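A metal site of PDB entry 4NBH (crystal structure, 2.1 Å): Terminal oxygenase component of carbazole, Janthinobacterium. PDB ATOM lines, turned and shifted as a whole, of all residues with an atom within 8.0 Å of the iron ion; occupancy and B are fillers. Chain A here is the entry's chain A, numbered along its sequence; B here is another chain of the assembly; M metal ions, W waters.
Three residues have an atom within 4 Å of the iron ion: His 183, His 187 and Asp 333.
The nearest printed residue that does not touch the iron ion is Asn 177 (4.3 Å).
OD2 of Asp 333 sits at hydrogen-bond distance from ND2 of Asn 330 (2.9 Å).
The backbone carbonyl oxygen (O) of Asp 333 lies close to the guanidinium group (NE) of Arg 337, 3.4 Å away.
A ring nitrogen (ND1) of His 187 lies close to the backbone carbonyl oxygen (O) of Phe 329 (3.4 Å).
ND1 of His 183 sits at hydrogen-bond distance from O of Asn 177, 3.0 Å away.
The backbone carbonyl oxygen (O) of Asp 180 is in hydrogen-bond range of a ring nitrogen (ND1) of His 183, at 2.6 Å.
OD1 of Asp 333 lies close to ND2 of Asn 177 (3.0 Å).
The iron ion is bound by water W1, OD1 of Asp 333, NE2 of His 183 and NE2 of His 187.
The iron ion has four donor atoms within binding distance.
Slightly farther from the iron ion lies water W2 (2.6 Å).
Slightly farther from the iron ion lies the side-chain carboxylate (OD2) of Asp 333 (2.7 Å).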
ATOM      1  N   ALA A 174      -0.980  -9.393 -18.600  1.00  0.00           N
ATOM      2  CA  ALA A 174      -1.189 -10.552 -17.736  1.00  0.00           C
ATOM      3  C   ALA A 174      -0.605 -10.292 -16.352  1.00  0.00           C
ATOM      4  O   ALA A 174      -1.260 -10.518 -15.328  1.00  0.00           O
ATOM      5  CB  ALA A 174      -0.537 -11.793 -18.358  1.00  0.00           C
ATOM      6  N   ASN A 177      -2.654  -7.616 -14.367  1.00  0.00           N
ATOM      7  CA  ASN A 177      -3.944  -8.101 -13.898  1.00  0.00           C
ATOM      8  C   ASN A 177      -3.727  -8.991 -12.683  1.00  0.00           C
ATOM      9  O   ASN A 177      -4.432  -8.884 -11.693  1.00  0.00           O
ATOM     10  CB  ASN A 177      -4.663  -8.912 -14.975  1.00  0.00           C
ATOM     11  CG  ASN A 177      -5.928  -9.565 -14.454  1.00  0.00           C
ATOM     12  OD1 ASN A 177      -6.915  -8.889 -14.167  1.00  0.00           O
ATOM     13  ND2 ASN A 177      -5.889 -10.876 -14.283  1.00  0.00           N
ATOM     14  N   GLY A 178      -2.734  -9.872 -12.761  1.00  0.00           N
ATOM     15  CA  GLY A 178      -2.459 -10.773 -11.660  1.00  0.00           C
ATOM     16  C   GLY A 178      -2.120 -10.099 -10.341  1.00  0.00           C
ATOM     17  O   GLY A 178      -2.581 -10.517  -9.279  1.00  0.00           O
ATOM     18  N   PHE A 179      -1.314  -9.039 -10.410  1.00  0.00           N
ATOM     19  CA  PHE A 179      -0.889  -8.314  -9.215  1.00  0.00           C
ATOM     20  C   PHE A 179      -1.846  -7.180  -8.820  1.00  0.00           C
ATOM     21  O   PHE A 179      -1.678  -6.545  -7.780  1.00  0.00           O
ATOM     22  CB  PHE A 179       0.527  -7.764  -9.473  1.00  0.00           C
ATOM     23  CG  PHE A 179       1.223  -7.252  -8.242  1.00  0.00           C
ATOM     24  CD1 PHE A 179       1.370  -8.060  -7.110  1.00  0.00           C
ATOM     25  CD2 PHE A 179       1.772  -5.972  -8.218  1.00  0.00           C
ATOM     26  CE1 PHE A 179       2.051  -7.597  -5.980  1.00  0.00           C
ATOM     27  CE2 PHE A 179       2.456  -5.501  -7.084  1.00  0.00           C
ATOM     28  CZ  PHE A 179       2.598  -6.320  -5.978  1.00  0.00           C
ATOM     29  N   ASP A 180      -2.869  -6.934  -9.644  1.00  0.00           N
ATOM     30  CA  ASP A 180      -3.884  -5.885  -9.429  1.00  0.00           C
ATOM     31  C   ASP A 180      -4.724  -6.183  -8.169  1.00  0.00           C
ATOM     32  O   ASP A 180      -5.540  -7.095  -8.170  1.00  0.00           O
ATOM     33  CB  ASP A 180      -4.798  -5.853 -10.650  1.00  0.00           C
ATOM     34  CG  ASP A 180      -5.718  -4.644 -10.692  1.00  0.00           C
ATOM     35  OD1 ASP A 180      -6.163  -4.181  -9.619  1.00  0.00           O
ATOM     36  OD2 ASP A 180      -5.988  -4.156 -11.810  1.00  0.00           O
ATOM     37  N   HIS A 183      -8.593  -6.099  -8.892  1.00  0.00           N
ATOM     38  CA  HIS A 183      -9.198  -6.949  -9.920  1.00  0.00           C
ATOM     39  C   HIS A 183      -9.955  -8.118  -9.292  1.00  0.00           C
ATOM     40  O   HIS A 183     -10.676  -8.845  -9.974  1.00  0.00           O
ATOM     41  CB  HIS A 183      -8.135  -7.473 -10.900  1.00  0.00           C
ATOM     42  CG  HIS A 183      -7.595  -8.824 -10.565  1.00  0.00           C
ATOM     43  ND1 HIS A 183      -6.631  -9.027  -9.595  1.00  0.00           N
ATOM     44  CD2 HIS A 183      -7.905 -10.049 -11.048  1.00  0.00           C
ATOM     45  CE1 HIS A 183      -6.367 -10.315  -9.494  1.00  0.00           C
ATOM     46  NE2 HIS A 183      -7.127 -10.952 -10.371  1.00  0.00           N
ATOM     47  N   ILE A 184      -9.786  -8.280  -7.982  1.00  0.00           N
ATOM     48  CA  ILE A 184     -10.443  -9.326  -7.223  1.00  0.00           C
ATOM     49  C   ILE A 184     -11.958  -9.296  -7.481  1.00  0.00           C
ATOM     50  O   ILE A 184     -12.656 -10.308  -7.357  1.00  0.00           O
ATOM     51  CB  ILE A 184     -10.138  -9.136  -5.715  1.00  0.00           C
ATOM     52  CG1 ILE A 184     -10.498 -10.380  -4.923  1.00  0.00           C
ATOM     53  CG2 ILE A 184     -10.909  -7.943  -5.171  1.00  0.00           C
ATOM     54  CD1 ILE A 184     -10.102 -10.272  -3.444  1.00  0.00           C
ATOM     55  N   TYR A 185     -12.455  -8.118  -7.858  1.00  0.00           N
ATOM     56  CA  TYR A 185     -13.875  -7.938  -8.155  1.00  0.00           C
ATOM     57  C   TYR A 185     -14.379  -8.903  -9.254  1.00  0.00           C
ATOM     58  O   TYR A 185     -15.525  -9.338  -9.211  1.00  0.00           O
ATOM     59  CB  TYR A 185     -14.130  -6.495  -8.616  1.00  0.00           C
ATOM     60  CG  TYR A 185     -15.586  -6.155  -8.865  1.00  0.00           C
ATOM     61  CD1 TYR A 185     -16.477  -5.938  -7.812  1.00  0.00           C
ATOM     62  CD2 TYR A 185     -16.087  -6.061 -10.170  1.00  0.00           C
ATOM     63  CE1 TYR A 185     -17.819  -5.638  -8.043  1.00  0.00           C
ATOM     64  CE2 TYR A 185     -17.432  -5.767 -10.414  1.00  0.00           C
ATOM     65  CZ  TYR A 185     -18.293  -5.555  -9.339  1.00  0.00           C
ATOM     66  OH  TYR A 185     -19.618  -5.267  -9.583  1.00  0.00           O
ATOM     67  N   ILE A 186     -13.525  -9.251 -10.215  1.00  0.00           N
ATOM     68  CA  ILE A 186     -13.947 -10.151 -11.286  1.00  0.00           C
ATOM     69  C   ILE A 186     -14.100 -11.601 -10.838  1.00  0.00           C
ATOM     70  O   ILE A 186     -14.623 -12.432 -11.580  1.00  0.00           O
ATOM     71  CB  ILE A 186     -12.965 -10.155 -12.495  1.00  0.00           C
ATOM     72  CG1 ILE A 186     -11.675 -10.894 -12.125  1.00  0.00           C
ATOM     73  CG2 ILE A 186     -12.650  -8.725 -12.926  1.00  0.00           C
ATOM     74  CD1 ILE A 186     -10.725 -11.115 -13.311  1.00  0.00           C
ATOM     75  N   HIS A 187     -13.640 -11.903  -9.625  1.00  0.00           N
ATOM     76  CA  HIS A 187     -13.701 -13.254  -9.064  1.00  0.00           C
ATOM     77  C   HIS A 187     -14.854 -13.468  -8.097  1.00  0.00           C
ATOM     78  O   HIS A 187     -14.982 -14.550  -7.528  1.00  0.00           O
ATOM     79  CB  HIS A 187     -12.399 -13.575  -8.326  1.00  0.00           C
ATOM     80  CG  HIS A 187     -11.201 -13.673  -9.222  1.00  0.00           C
ATOM     81  ND1 HIS A 187     -11.120 -14.565 -10.271  1.00  0.00           N
ATOM     82  CD2 HIS A 187     -10.024 -12.991  -9.214  1.00  0.00           C
ATOM     83  CE1 HIS A 187      -9.953 -14.426 -10.872  1.00  0.00           C
ATOM     84  NE2 HIS A 187      -9.265 -13.483 -10.250  1.00  0.00           N
ATOM     85  N   LEU A 270       3.955 -14.452 -10.555  1.00  0.00           N
ATOM     86  CA  LEU A 270       3.220 -14.102  -9.352  1.00  0.00           C
ATOM     87  C   LEU A 270       3.176 -15.237  -8.352  1.00  0.00           C
ATOM     88  O   LEU A 270       3.100 -16.411  -8.736  1.00  0.00           O
ATOM     89  CB  LEU A 270       1.783 -13.722  -9.734  1.00  0.00           C
ATOM     90  CG  LEU A 270       0.871 -13.189  -8.623  1.00  0.00           C
ATOM     91  CD1 LEU A 270       1.117 -11.703  -8.430  1.00  0.00           C
ATOM     92  CD2 LEU A 270      -0.597 -13.420  -8.993  1.00  0.00           C
ATOM     93  N   PHE A 275      -2.800 -20.453  -1.383  1.00  0.00           N
ATOM     94  CA  PHE A 275      -3.852 -20.475  -2.390  1.00  0.00           C
ATOM     95  C   PHE A 275      -3.799 -21.802  -3.140  1.00  0.00           C
ATOM     96  O   PHE A 275      -2.722 -22.310  -3.418  1.00  0.00           O
ATOM     97  CB  PHE A 275      -3.647 -19.325  -3.383  1.00  0.00           C
ATOM     98  CG  PHE A 275      -4.841 -19.056  -4.255  1.00  0.00           C
ATOM     99  CD1 PHE A 275      -5.897 -18.268  -3.791  1.00  0.00           C
ATOM    100  CD2 PHE A 275      -4.932 -19.595  -5.543  1.00  0.00           C
ATOM    101  CE1 PHE A 275      -7.012 -18.015  -4.588  1.00  0.00           C
ATOM    102  CE2 PHE A 275      -6.039 -19.354  -6.343  1.00  0.00           C
ATOM    103  CZ  PHE A 275      -7.084 -18.563  -5.866  1.00  0.00           C
ATOM    104  N   GLU A 284       2.342 -18.390 -10.751  1.00  0.00           N
ATOM    105  CA  GLU A 284       1.986 -18.365 -12.173  1.00  0.00           C
ATOM    106  C   GLU A 284       2.862 -17.389 -12.948  1.00  0.00           C
ATOM    107  O   GLU A 284       3.046 -16.234 -12.540  1.00  0.00           O
ATOM    108  CB  GLU A 284       0.494 -18.041 -12.377  1.00  0.00           C
ATOM    109  CG  GLU A 284      -0.013 -16.807 -11.640  1.00  0.00           C
ATOM    110  CD  GLU A 284      -1.420 -16.396 -12.072  1.00  0.00           C
ATOM    111  OE1 GLU A 284      -2.282 -17.279 -12.246  1.00  0.00           O
ATOM    112  OE2 GLU A 284      -1.666 -15.189 -12.240  1.00  0.00           O
ATOM    113  N   TYR A 286       3.860 -15.489 -16.723  1.00  0.00           N
ATOM    114  CA  TYR A 286       3.243 -14.936 -17.922  1.00  0.00           C
ATOM    115  C   TYR A 286       4.467 -14.763 -18.833  1.00  0.00           C
ATOM    116  O   TYR A 286       5.122 -13.728 -18.827  1.00  0.00           O
ATOM    117  CB  TYR A 286       2.612 -13.571 -17.616  1.00  0.00           C
ATOM    118  CG  TYR A 286       1.898 -13.513 -16.285  1.00  0.00           C
ATOM    119  CD1 TYR A 286       0.636 -14.065 -16.120  1.00  0.00           C
ATOM    120  CD2 TYR A 286       2.518 -12.937 -15.175  1.00  0.00           C
ATOM    121  CE1 TYR A 286      -0.013 -14.030 -14.875  1.00  0.00           C
ATOM    122  CE2 TYR A 286       1.881 -12.895 -13.927  1.00  0.00           C
ATOM    123  CZ  TYR A 286       0.619 -13.448 -13.794  1.00  0.00           C
ATOM    124  OH  TYR A 286      -0.024 -13.391 -12.584  1.00  0.00           O
ATOM    125  N   TYR A 296       0.749 -19.004 -20.263  1.00  0.00           N
ATOM    126  CA  TYR A 296       0.157 -18.778 -18.952  1.00  0.00           C
ATOM    127  C   TYR A 296       0.507 -20.083 -18.238  1.00  0.00           C
ATOM    128  O   TYR A 296      -0.262 -21.046 -18.262  1.00  0.00           O
ATOM    129  CB  TYR A 296      -1.361 -18.585 -19.073  1.00  0.00           C
ATOM    130  CG  TYR A 296      -2.066 -18.349 -17.757  1.00  0.00           C
ATOM    131  CD1 TYR A 296      -1.420 -17.681 -16.711  1.00  0.00           C
ATOM    132  CD2 TYR A 296      -3.378 -18.755 -17.560  1.00  0.00           C
ATOM    133  CE1 TYR A 296      -2.077 -17.420 -15.510  1.00  0.00           C
ATOM    134  CE2 TYR A 296      -4.050 -18.505 -16.374  1.00  0.00           C
ATOM    135  CZ  TYR A 296      -3.393 -17.835 -15.347  1.00  0.00           C
ATOM    136  OH  TYR A 296      -4.054 -17.588 -14.162  1.00  0.00           O
ATOM    137  N   PHE A 329     -11.218 -20.599 -11.254  1.00  0.00           N
ATOM    138  CA  PHE A 329     -10.943 -19.282 -10.724  1.00  0.00           C
ATOM    139  C   PHE A 329     -10.254 -18.400 -11.765  1.00  0.00           C
ATOM    140  O   PHE A 329     -10.800 -17.390 -12.189  1.00  0.00           O
ATOM    141  CB  PHE A 329     -10.064 -19.400  -9.480  1.00  0.00           C
ATOM    142  CG  PHE A 329      -9.908 -18.107  -8.714  1.00  0.00           C
ATOM    143  CD1 PHE A 329     -10.879 -17.693  -7.815  1.00  0.00           C
ATOM    144  CD2 PHE A 329      -8.760 -17.337  -8.870  1.00  0.00           C
ATOM    145  CE1 PHE A 329     -10.718 -16.530  -7.059  1.00  0.00           C
ATOM    146  CE2 PHE A 329      -8.577 -16.168  -8.121  1.00  0.00           C
ATOM    147  CZ  PHE A 329      -9.561 -15.762  -7.215  1.00  0.00           C
ATOM    148  N   ASN A 330      -9.058 -18.814 -12.193  1.00  0.00           N
ATOM    149  CA  ASN A 330      -8.263 -18.039 -13.145  1.00  0.00           C
ATOM    150  C   ASN A 330      -8.797 -17.873 -14.567  1.00  0.00           C
ATOM    151  O   ASN A 330      -8.276 -17.044 -15.312  1.00  0.00           O
ATOM    152  CB  ASN A 330      -6.841 -18.589 -13.209  1.00  0.00           C
ATOM    153  CG  ASN A 330      -6.144 -18.513 -11.865  1.00  0.00           C
ATOM    154  OD1 ASN A 330      -5.766 -19.534 -11.300  1.00  0.00           O
ATOM    155  ND2 ASN A 330      -5.973 -17.304 -11.346  1.00  0.00           N
ATOM    156  N   ASN A 331      -9.798 -18.647 -14.969  1.00  0.00           N
ATOM    157  CA  ASN A 331     -10.320 -18.478 -16.316  1.00  0.00           C
ATOM    158  C   ASN A 331     -10.811 -17.038 -16.534  1.00  0.00           C
ATOM    159  O   ASN A 331     -10.712 -16.499 -17.637  1.00  0.00           O
ATOM    160  CB  ASN A 331     -11.445 -19.472 -16.609  1.00  0.00           C
ATOM    161  CG  ASN A 331     -10.924 -20.770 -17.208  1.00  0.00           C
ATOM    162  OD1 ASN A 331      -9.723 -20.925 -17.436  1.00  0.00           O
ATOM    163  ND2 ASN A 331     -11.823 -21.702 -17.463  1.00  0.00           N
ATOM    164  N   ASP A 332     -11.346 -16.418 -15.491  1.00  0.00           N
ATOM    165  CA  ASP A 332     -11.814 -15.047 -15.624  1.00  0.00           C
ATOM    166  C   ASP A 332     -10.641 -14.080 -15.830  1.00  0.00           C
ATOM    167  O   ASP A 332     -10.825 -12.998 -16.392  1.00  0.00           O
ATOM    168  CB  ASP A 332     -12.629 -14.611 -14.410  1.00  0.00           C
ATOM    169  CG  ASP A 332     -13.985 -15.268 -14.371  1.00  0.00           C
ATOM    170  OD1 ASP A 332     -14.637 -15.308 -15.447  1.00  0.00           O
ATOM    171  OD2 ASP A 332     -14.414 -15.722 -13.298  1.00  0.00           O
ATOM    172  N   ASP A 333      -9.456 -14.466 -15.376  1.00  0.00           N
ATOM    173  CA  ASP A 333      -8.259 -13.635 -15.529  1.00  0.00           C
ATOM    174  C   ASP A 333      -7.858 -13.619 -16.999  1.00  0.00           C
ATOM    175  O   ASP A 333      -7.345 -12.616 -17.509  1.00  0.00           O
ATOM    176  CB  ASP A 333      -7.093 -14.179 -14.695  1.00  0.00           C
ATOM    177  CG  ASP A 333      -7.305 -14.013 -13.215  1.00  0.00           C
ATOM    178  OD1 ASP A 333      -7.473 -12.854 -12.771  1.00  0.00           O
ATOM    179  OD2 ASP A 333      -7.309 -15.031 -12.490  1.00  0.00           O
ATOM    180  N   ILE A 334      -8.091 -14.748 -17.665  1.00  0.00           N
ATOM    181  CA  ILE A 334      -7.749 -14.865 -19.078  1.00  0.00           C
ATOM    182  C   ILE A 334      -8.524 -13.868 -19.935  1.00  0.00           C
ATOM    183  O   ILE A 334      -7.908 -13.110 -20.684  1.00  0.00           O
ATOM    184  CB  ILE A 334      -7.998 -16.309 -19.584  1.00  0.00           C
ATOM    185  CG1 ILE A 334      -6.973 -17.257 -18.954  1.00  0.00           C
ATOM    186  CG2 ILE A 334      -7.905 -16.348 -21.106  1.00  0.00           C
ATOM    187  CD1 ILE A 334      -7.273 -18.747 -19.184  1.00  0.00           C
ATOM    188  N   ALA A 336     -10.080 -11.242 -18.928  1.00  0.00           N
ATOM    189  CA  ALA A 336      -9.868  -9.890 -18.412  1.00  0.00           C
ATOM    190  C   ALA A 336      -8.627  -9.277 -19.085  1.00  0.00           C
ATOM    191  O   ALA A 336      -8.652  -8.121 -19.515  1.00  0.00           O
ATOM    192  CB  ALA A 336      -9.680  -9.926 -16.881  1.00  0.00           C
ATOM    193  N   ARG A 337      -7.559 -10.077 -19.174  1.00  0.00           N
ATOM    194  CA  ARG A 337      -6.319  -9.648 -19.822  1.00  0.00           C
ATOM    195  C   ARG A 337      -6.608  -9.283 -21.266  1.00  0.00           C
ATOM    196  O   ARG A 337      -6.124  -8.272 -21.776  1.00  0.00           O
ATOM    197  CB  ARG A 337      -5.284 -10.778 -19.883  1.00  0.00           C
ATOM    198  CG  ARG A 337      -4.874 -11.332 -18.564  1.00  0.00           C
ATOM    199  CD  ARG A 337      -4.020 -12.578 -18.771  1.00  0.00           C
ATOM    200  NE  ARG A 337      -4.045 -13.336 -17.543  1.00  0.00           N
ATOM    201  CZ  ARG A 337      -3.555 -14.561 -17.403  1.00  0.00           C
ATOM    202  NH1 ARG A 337      -2.994 -15.199 -18.418  1.00  0.00           N
ATOM    203  NH2 ARG A 337      -3.660 -15.158 -16.223  1.00  0.00           N
ATOM    204  N   TYR B  92     -14.645  -4.903 -14.434  1.00  0.00           N
ATOM    205  CA  TYR B  92     -13.256  -5.088 -14.004  1.00  0.00           C
ATOM    206  C   TYR B  92     -12.957  -4.629 -12.568  1.00  0.00           C
ATOM    207  O   TYR B  92     -12.663  -5.453 -11.704  1.00  0.00           O
ATOM    208  CB  TYR B  92     -12.317  -4.387 -14.989  1.00  0.00           C
ATOM    209  CG  TYR B  92     -10.946  -5.002 -15.142  1.00  0.00           C
ATOM    210  CD1 TYR B  92     -10.498  -6.013 -14.284  1.00  0.00           C
ATOM    211  CD2 TYR B  92     -10.063  -4.532 -16.111  1.00  0.00           C
ATOM    212  CE1 TYR B  92      -9.206  -6.543 -14.394  1.00  0.00           C
ATOM    213  CE2 TYR B  92      -8.777  -5.047 -16.227  1.00  0.00           C
ATOM    214  CZ  TYR B  92      -8.354  -6.037 -15.375  1.00  0.00           C
ATOM    215  OH  TYR B  92      -7.066  -6.510 -15.488  1.00  0.00           O
HETATM  216 FE    FE M   1      -7.370 -12.917 -10.802  1.00  0.00          FE
HETATM  217  O   HOH W   1      -5.695 -13.755 -10.665  1.00  0.00           O
HETATM  218  O   HOH W   2      -6.168 -13.446  -8.517  1.00  0.00           O
